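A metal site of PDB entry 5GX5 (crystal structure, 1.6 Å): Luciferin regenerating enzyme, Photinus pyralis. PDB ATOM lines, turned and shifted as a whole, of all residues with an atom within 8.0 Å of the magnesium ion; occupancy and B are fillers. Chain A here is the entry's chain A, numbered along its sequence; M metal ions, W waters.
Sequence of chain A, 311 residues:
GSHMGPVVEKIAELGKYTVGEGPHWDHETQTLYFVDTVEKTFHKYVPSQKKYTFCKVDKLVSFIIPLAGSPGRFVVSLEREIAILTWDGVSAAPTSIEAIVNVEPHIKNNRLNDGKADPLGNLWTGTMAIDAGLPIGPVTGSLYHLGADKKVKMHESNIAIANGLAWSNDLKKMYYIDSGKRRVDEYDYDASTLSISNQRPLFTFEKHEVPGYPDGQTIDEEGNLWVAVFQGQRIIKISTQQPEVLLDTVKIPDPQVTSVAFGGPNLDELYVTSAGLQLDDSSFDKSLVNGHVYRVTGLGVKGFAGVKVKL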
ATOM      1  N   VAL A  19      12.161  -8.307  11.744  1.00  0.00           N
ATOM      2  CA  VAL A  19      13.430  -8.924  12.105  1.00  0.00           C
ATOM      3  C   VAL A  19      13.938  -8.237  13.368  1.00  0.00           C
ATOM      4  O   VAL A  19      14.717  -7.274  13.298  1.00  0.00           O
ATOM      5  CB  VAL A  19      14.485  -8.833  10.986  1.00  0.00           C
ATOM      6  CG1 VAL A  19      15.731  -9.626  11.373  1.00  0.00           C
ATOM      7  CG2 VAL A  19      13.937  -9.343   9.641  1.00  0.00           C
ATOM      8  N   GLY A  20      13.491  -8.703  14.529  1.00  0.00           N
ATOM      9  CA  GLY A  20      14.036  -8.213  15.785  1.00  0.00           C
ATOM     10  C   GLY A  20      15.458  -8.718  15.976  1.00  0.00           C
ATOM     11  O   GLY A  20      15.766  -9.871  15.654  1.00  0.00           O
ATOM     12  N   GLU A  21      16.315  -7.862  16.499  1.00  0.00           N
ATOM     13  CA  GLU A  21      17.765  -8.105  16.468  1.00  0.00           C
ATOM     14  C   GLU A  21      18.486  -7.204  17.469  1.00  0.00           C
ATOM     15  O   GLU A  21      17.892  -6.310  18.076  1.00  0.00           O
ATOM     16  CB  GLU A  21      18.316  -7.867  15.059  1.00  0.00           C
ATOM     17  CG  GLU A  21      18.557  -9.121  14.270  1.00  0.00           C
ATOM     18  CD  GLU A  21      19.903  -9.719  14.595  1.00  0.00           C
ATOM     19  OE1 GLU A  21      20.330 -10.641  13.837  1.00  0.00           O
ATOM     20  OE2 GLU A  21      20.548  -9.262  15.585  1.00  0.00           O
ATOM     21  N   GLY A  22      19.794  -7.443  17.602  1.00  0.00           N
ATOM     22  CA  GLY A  22      20.686  -6.625  18.385  1.00  0.00           C
ATOM     23  C   GLY A  22      20.267  -6.310  19.827  1.00  0.00           C
ATOM     24  O   GLY A  22      20.326  -5.152  20.250  1.00  0.00           O
ATOM     25  N   PRO A  23      19.885  -7.319  20.610  1.00  0.00           N
ATOM     26  CA  PRO A  23      19.494  -7.029  22.004  1.00  0.00           C
ATOM     27  C   PRO A  23      20.686  -6.610  22.842  1.00  0.00           C
ATOM     28  O   PRO A  23      21.780  -7.192  22.740  1.00  0.00           O
ATOM     29  CB  PRO A  23      18.910  -8.356  22.490  1.00  0.00           C
ATOM     30  CG  PRO A  23      19.651  -9.388  21.696  1.00  0.00           C
ATOM     31  CD  PRO A  23      19.817  -8.755  20.318  1.00  0.00           C
ATOM     32  N   THR A  37      15.831  -4.754  12.036  1.00  0.00           N
ATOM     33  CA  THR A  37      16.831  -4.461  11.019  1.00  0.00           C
ATOM     34  C   THR A  37      16.227  -4.233   9.641  1.00  0.00           C
ATOM     35  O   THR A  37      16.957  -3.875   8.721  1.00  0.00           O
ATOM     36  CB  THR A  37      17.882  -5.580  10.973  1.00  0.00           C
ATOM     37  OG1 THR A  37      17.245  -6.832  10.662  1.00  0.00           O
ATOM     38  CG2 THR A  37      18.563  -5.708  12.310  1.00  0.00           C
ATOM     39  N   SER A  62      21.002  -1.646  12.607  1.00  0.00           N
ATOM     40  CA  SER A  62      21.319  -3.008  13.003  1.00  0.00           C
ATOM     41  C   SER A  62      21.860  -3.177  14.412  1.00  0.00           C
ATOM     42  O   SER A  62      21.976  -4.315  14.857  1.00  0.00           O
ATOM     43  CB  SER A  62      22.338  -3.594  12.014  1.00  0.00           C
ATOM     44  OG  SER A  62      23.551  -2.850  12.106  1.00  0.00           O
ATOM     45  N   ASN A 113      25.695  -4.740   9.769  1.00  0.00           N
ATOM     46  CA  ASN A 113      24.830  -5.697  10.439  1.00  0.00           C
ATOM     47  C   ASN A 113      25.185  -5.744  11.928  1.00  0.00           C
ATOM     48  O   ASN A 113      25.211  -4.689  12.577  1.00  0.00           O
ATOM     49  CB  ASN A 113      24.927  -7.087   9.794  1.00  0.00           C
ATOM     50  CG  ASN A 113      23.718  -7.947  10.108  1.00  0.00           C
ATOM     51  OD1 ASN A 113      22.620  -7.416  10.374  1.00  0.00           O
ATOM     52  ND2 ASN A 113      23.878  -9.278  10.080  1.00  0.00           N
ATOM     53  N   ASP A 114      25.515  -6.915  12.484  1.00  0.00           N
ATOM     54  CA  ASP A 114      25.651  -7.028  13.926  1.00  0.00           C
ATOM     55  C   ASP A 114      26.852  -6.211  14.429  1.00  0.00           C
ATOM     56  O   ASP A 114      27.892  -6.134  13.769  1.00  0.00           O
ATOM     57  CB  ASP A 114      25.796  -8.495  14.354  1.00  0.00           C
ATOM     58  CG  ASP A 114      25.050  -8.813  15.675  1.00  0.00           C
ATOM     59  OD1 ASP A 114      24.607  -7.840  16.356  1.00  0.00           O
ATOM     60  OD2 ASP A 114      24.898 -10.011  16.057  1.00  0.00           O
ATOM     61  N   GLY A 115      26.681  -5.600  15.599  1.00  0.00           N
ATOM     62  CA  GLY A 115      27.770  -4.892  16.245  1.00  0.00           C
ATOM     63  C   GLY A 115      27.666  -5.042  17.750  1.00  0.00           C
ATOM     64  O   GLY A 115      26.574  -5.197  18.314  1.00  0.00           O
ATOM     65  N   MET A 128      27.655  -6.302   5.138  1.00  0.00           N
ATOM     66  CA  MET A 128      27.143  -7.335   4.237  1.00  0.00           C
ATOM     67  C   MET A 128      26.360  -6.660   3.122  1.00  0.00           C
ATOM     68  O   MET A 128      25.963  -5.505   3.244  1.00  0.00           O
ATOM     69  CB  MET A 128      26.252  -8.328   4.974  1.00  0.00           C
ATOM     70  CG  MET A 128      25.086  -7.651   5.657  1.00  0.00           C
ATOM     71  SD  MET A 128      24.049  -8.844   6.506  1.00  0.00           S
ATOM     72  CE  MET A 128      23.062  -9.434   5.136  1.00  0.00           C
ATOM     73  N   ILE A 161      27.238 -12.947   5.584  1.00  0.00           N
ATOM     74  CA  ILE A 161      26.286 -12.333   6.492  1.00  0.00           C
ATOM     75  C   ILE A 161      26.999 -12.152   7.823  1.00  0.00           C
ATOM     76  O   ILE A 161      27.131 -13.101   8.609  1.00  0.00           O
ATOM     77  CB  ILE A 161      25.001 -13.160   6.636  1.00  0.00           C
ATOM     78  CG1 ILE A 161      24.250 -13.159   5.305  1.00  0.00           C
ATOM     79  CG2 ILE A 161      24.105 -12.580   7.727  1.00  0.00           C
ATOM     80  CD1 ILE A 161      22.904 -13.857   5.352  1.00  0.00           C
ATOM     81  N   ALA A 162      27.451 -10.923   8.091  1.00  0.00           N
ATOM     82  CA  ALA A 162      28.154 -10.607   9.329  1.00  0.00           C
ATOM     83  C   ALA A 162      27.226 -10.732  10.538  1.00  0.00           C
ATOM     84  O   ALA A 162      26.239 -10.003  10.635  1.00  0.00           O
ATOM     85  CB  ALA A 162      28.699  -9.183   9.229  1.00  0.00           C
ATOM     86  N   ASN A 163      27.532 -11.633  11.466  1.00  0.00           N
ATOM     87  CA  ASN A 163      26.624 -11.767  12.602  1.00  0.00           C
ATOM     88  C   ASN A 163      27.318 -11.800  13.961  1.00  0.00           C
ATOM     89  O   ASN A 163      28.159 -10.941  14.232  1.00  0.00           O
ATOM     90  CB  ASN A 163      25.715 -12.972  12.374  1.00  0.00           C
ATOM     91  CG  ASN A 163      24.341 -12.531  11.996  1.00  0.00           C
ATOM     92  OD1 ASN A 163      23.823 -11.585  12.599  1.00  0.00           O
ATOM     93  ND2 ASN A 163      23.756 -13.130  10.969  1.00  0.00           N
ATOM     94  N   GLY A 164      26.952 -12.735  14.836  1.00  0.00           N
ATOM     95  CA  GLY A 164      27.223 -12.560  16.256  1.00  0.00           C
ATOM     96  C   GLY A 164      28.705 -12.574  16.624  1.00  0.00           C
ATOM     97  O   GLY A 164      29.520 -13.238  15.991  1.00  0.00           O
ATOM     98  N   ILE A 177      30.648 -15.217  13.956  1.00  0.00           N
ATOM     99  CA  ILE A 177      29.728 -15.967  13.102  1.00  0.00           C
ATOM    100  C   ILE A 177      29.548 -15.219  11.795  1.00  0.00           C
ATOM    101  O   ILE A 177      29.013 -14.103  11.788  1.00  0.00           O
ATOM    102  CB  ILE A 177      28.377 -16.189  13.793  1.00  0.00           C
ATOM    103  CG1 ILE A 177      28.572 -17.106  14.994  1.00  0.00           C
ATOM    104  CG2 ILE A 177      27.361 -16.746  12.775  1.00  0.00           C
ATOM    105  CD1 ILE A 177      27.388 -17.070  15.974  1.00  0.00           C
ATOM    106  N   SER A 179      27.113 -16.195   9.006  1.00  0.00           N
ATOM    107  CA  SER A 179      26.021 -17.164   8.937  1.00  0.00           C
ATOM    108  C   SER A 179      26.157 -18.072   7.716  1.00  0.00           C
ATOM    109  O   SER A 179      25.798 -19.260   7.783  1.00  0.00           O
ATOM    110  CB  SER A 179      24.673 -16.451   8.925  1.00  0.00           C
ATOM    111  OG  SER A 179      24.495 -15.709  10.109  1.00  0.00           O
ATOM    112  N   PRO A 214      23.635 -20.237  12.038  1.00  0.00           N
ATOM    113  CA  PRO A 214      23.968 -19.472  13.246  1.00  0.00           C
ATOM    114  C   PRO A 214      23.776 -17.986  12.986  1.00  0.00           C
ATOM    115  O   PRO A 214      24.063 -17.485  11.897  1.00  0.00           O
ATOM    116  CB  PRO A 214      25.439 -19.840  13.504  1.00  0.00           C
ATOM    117  CG  PRO A 214      25.990 -20.131  12.144  1.00  0.00           C
ATOM    118  CD  PRO A 214      24.838 -20.785  11.373  1.00  0.00           C
ATOM    119  N   ASP A 215      23.263 -17.290  13.993  1.00  0.00           N
ATOM    120  CA  ASP A 215      22.982 -15.861  13.836  1.00  0.00           C
ATOM    121  C   ASP A 215      23.685 -15.123  14.974  1.00  0.00           C
ATOM    122  O   ASP A 215      24.913 -15.021  14.947  1.00  0.00           O
ATOM    123  CB  ASP A 215      21.468 -15.633  13.806  1.00  0.00           C
ATOM    124  CG  ASP A 215      21.063 -14.240  13.275  1.00  0.00           C
ATOM    125  OD1 ASP A 215      21.873 -13.280  13.318  1.00  0.00           O
ATOM    126  OD2 ASP A 215      19.900 -14.090  12.803  1.00  0.00           O
ATOM    127  N   GLY A 216      22.950 -14.635  15.979  1.00  0.00           N
ATOM    128  CA  GLY A 216      23.599 -13.975  17.095  1.00  0.00           C
ATOM    129  C   GLY A 216      24.161 -14.972  18.106  1.00  0.00           C
ATOM    130  O   GLY A 216      23.820 -16.144  18.113  1.00  0.00           O
ATOM    131  N   GLN A 217      25.050 -14.475  18.979  1.00  0.00           N
ATOM    132  CA  GLN A 217      25.582 -15.313  20.039  1.00  0.00           C
ATOM    133  C   GLN A 217      25.967 -14.453  21.232  1.00  0.00           C
ATOM    134  O   GLN A 217      26.168 -13.237  21.123  1.00  0.00           O
ATOM    135  CB  GLN A 217      26.804 -16.126  19.571  1.00  0.00           C
ATOM    136  CG  GLN A 217      28.052 -15.300  19.253  1.00  0.00           C
ATOM    137  CD  GLN A 217      29.206 -16.202  18.841  1.00  0.00           C
ATOM    138  OE1 GLN A 217      29.219 -17.403  19.161  1.00  0.00           O
ATOM    139  NE2 GLN A 217      30.165 -15.648  18.096  1.00  0.00           N
ATOM    140  N   ALA A 228      22.001 -18.348  18.667  1.00  0.00           N
ATOM    141  CA  ALA A 228      20.680 -18.365  18.057  1.00  0.00           C
ATOM    142  C   ALA A 228      20.737 -19.107  16.730  1.00  0.00           C
ATOM    143  O   ALA A 228      21.663 -18.914  15.943  1.00  0.00           O
ATOM    144  CB  ALA A 228      20.201 -16.933  17.839  1.00  0.00           C
ATOM    145  N   PHE A 230      18.904 -19.495  13.314  1.00  0.00           N
ATOM    146  CA  PHE A 230      17.906 -18.997  12.387  1.00  0.00           C
ATOM    147  C   PHE A 230      17.440 -20.128  11.468  1.00  0.00           C
ATOM    148  O   PHE A 230      18.263 -20.798  10.846  1.00  0.00           O
ATOM    149  CB  PHE A 230      18.508 -17.840  11.582  1.00  0.00           C
ATOM    150  CG  PHE A 230      17.523 -17.131  10.714  1.00  0.00           C
ATOM    151  CD1 PHE A 230      16.847 -15.989  11.170  1.00  0.00           C
ATOM    152  CD2 PHE A 230      17.265 -17.576   9.429  1.00  0.00           C
ATOM    153  CE1 PHE A 230      15.933 -15.318  10.337  1.00  0.00           C
ATOM    154  CE2 PHE A 230      16.337 -16.914   8.611  1.00  0.00           C
ATOM    155  CZ  PHE A 230      15.680 -15.798   9.062  1.00  0.00           C
ATOM    156  N   VAL A 257      14.967 -17.663  14.943  1.00  0.00           N
ATOM    157  CA  VAL A 257      15.641 -17.070  16.087  1.00  0.00           C
ATOM    158  C   VAL A 257      16.836 -16.260  15.591  1.00  0.00           C
ATOM    159  O   VAL A 257      17.646 -16.770  14.816  1.00  0.00           O
ATOM    160  CB  VAL A 257      16.110 -18.171  17.057  1.00  0.00           C
ATOM    161  CG1 VAL A 257      16.661 -17.544  18.302  1.00  0.00           C
ATOM    162  CG2 VAL A 257      14.957 -19.114  17.379  1.00  0.00           C
ATOM    163  N   THR A 258      16.950 -15.005  16.051  1.00  0.00           N
ATOM    164  CA  THR A 258      17.981 -14.100  15.535  1.00  0.00           C
ATOM    165  C   THR A 258      19.074 -13.748  16.534  1.00  0.00           C
ATOM    166  O   THR A 258      20.235 -13.607  16.124  1.00  0.00           O
ATOM    167  CB  THR A 258      17.360 -12.801  15.007  1.00  0.00           C
ATOM    168  OG1 THR A 258      16.655 -12.140  16.070  1.00  0.00           O
ATOM    169  CG2 THR A 258      16.378 -13.070  13.874  1.00  0.00           C
ATOM    170  N   SER A 259      18.772 -13.525  17.810  1.00  0.00           N
ATOM    171  CA  SER A 259      19.850 -13.162  18.723  1.00  0.00           C
ATOM    172  C   SER A 259      19.441 -13.443  20.169  1.00  0.00           C
ATOM    173  O   SER A 259      18.302 -13.817  20.459  1.00  0.00           O
ATOM    174  CB  SER A 259      20.286 -11.698  18.560  1.00  0.00           C
ATOM    175  OG  SER A 259      21.625 -11.510  19.084  1.00  0.00           O
ATOM    176  N   THR A 273      15.405 -12.760  20.607  1.00  0.00           N
ATOM    177  CA  THR A 273      14.665 -12.107  19.525  1.00  0.00           C
ATOM    178  C   THR A 273      14.486 -13.067  18.349  1.00  0.00           C
ATOM    179  O   THR A 273      15.249 -14.021  18.171  1.00  0.00           O
ATOM    180  CB  THR A 273      15.400 -10.849  19.042  1.00  0.00           C
ATOM    181  OG1 THR A 273      16.727 -11.204  18.660  1.00  0.00           O
ATOM    182  CG2 THR A 273      15.462  -9.802  20.163  1.00  0.00           C
HETATM  183 MG    MG M   1      22.058 -11.119  13.370  1.00  0.00          MG
HETATM  184  O   HOH W   1      22.549  -9.073  13.315  1.00  0.00           O
HETATM  185  O   HOH W   2      21.359 -10.934  11.395  1.00  0.00           O
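ND2 of Asn 113 lies close to OD1 of Asn 163 (3.4 Å).
The side-chain hydroxyl (OG) of Ser 179 sits at hydrogen-bond distance from the side-chain amide nitrogen (ND2) of Asn 163 (2.8 Å).
N of Asn 163 lies within hydrogen-bond range of O of Ile 177 (2.9 Å).
The backbone NH (N) of Gly 164 lies within hydrogen-bond range of the backbone carbonyl oxygen (O) of Asp 215 (3.1 Å).
N of Asp 215 lies within hydrogen-bond range of O of Ala 228 (3.0 Å).
Three residues have an atom within 4 Å of the magnesium ion: Glu 21, Asn 163 and Asp 215.
The magnesium ion is bound by the side-chain carboxylate of Glu 21 (1.9 Å), the side-chain amide oxygen of Asn 163 (2.0 Å), water W2 (2.1 Å), water W1 (2.1 Å) and the side-chain carboxylate of Asp 215 (2.2 Å).
The magnesium ion has five donor atoms within binding distance.
Water W1 bridges OE2 of Glu 21 (3.0 Å) and OD1 of Asn 113 (3.4 Å).
Water W2 lies within hydrogen-bond range of ND2 of Asn 163 (3.3 Å) and ND2 of Asn 113 (3.3 Å).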
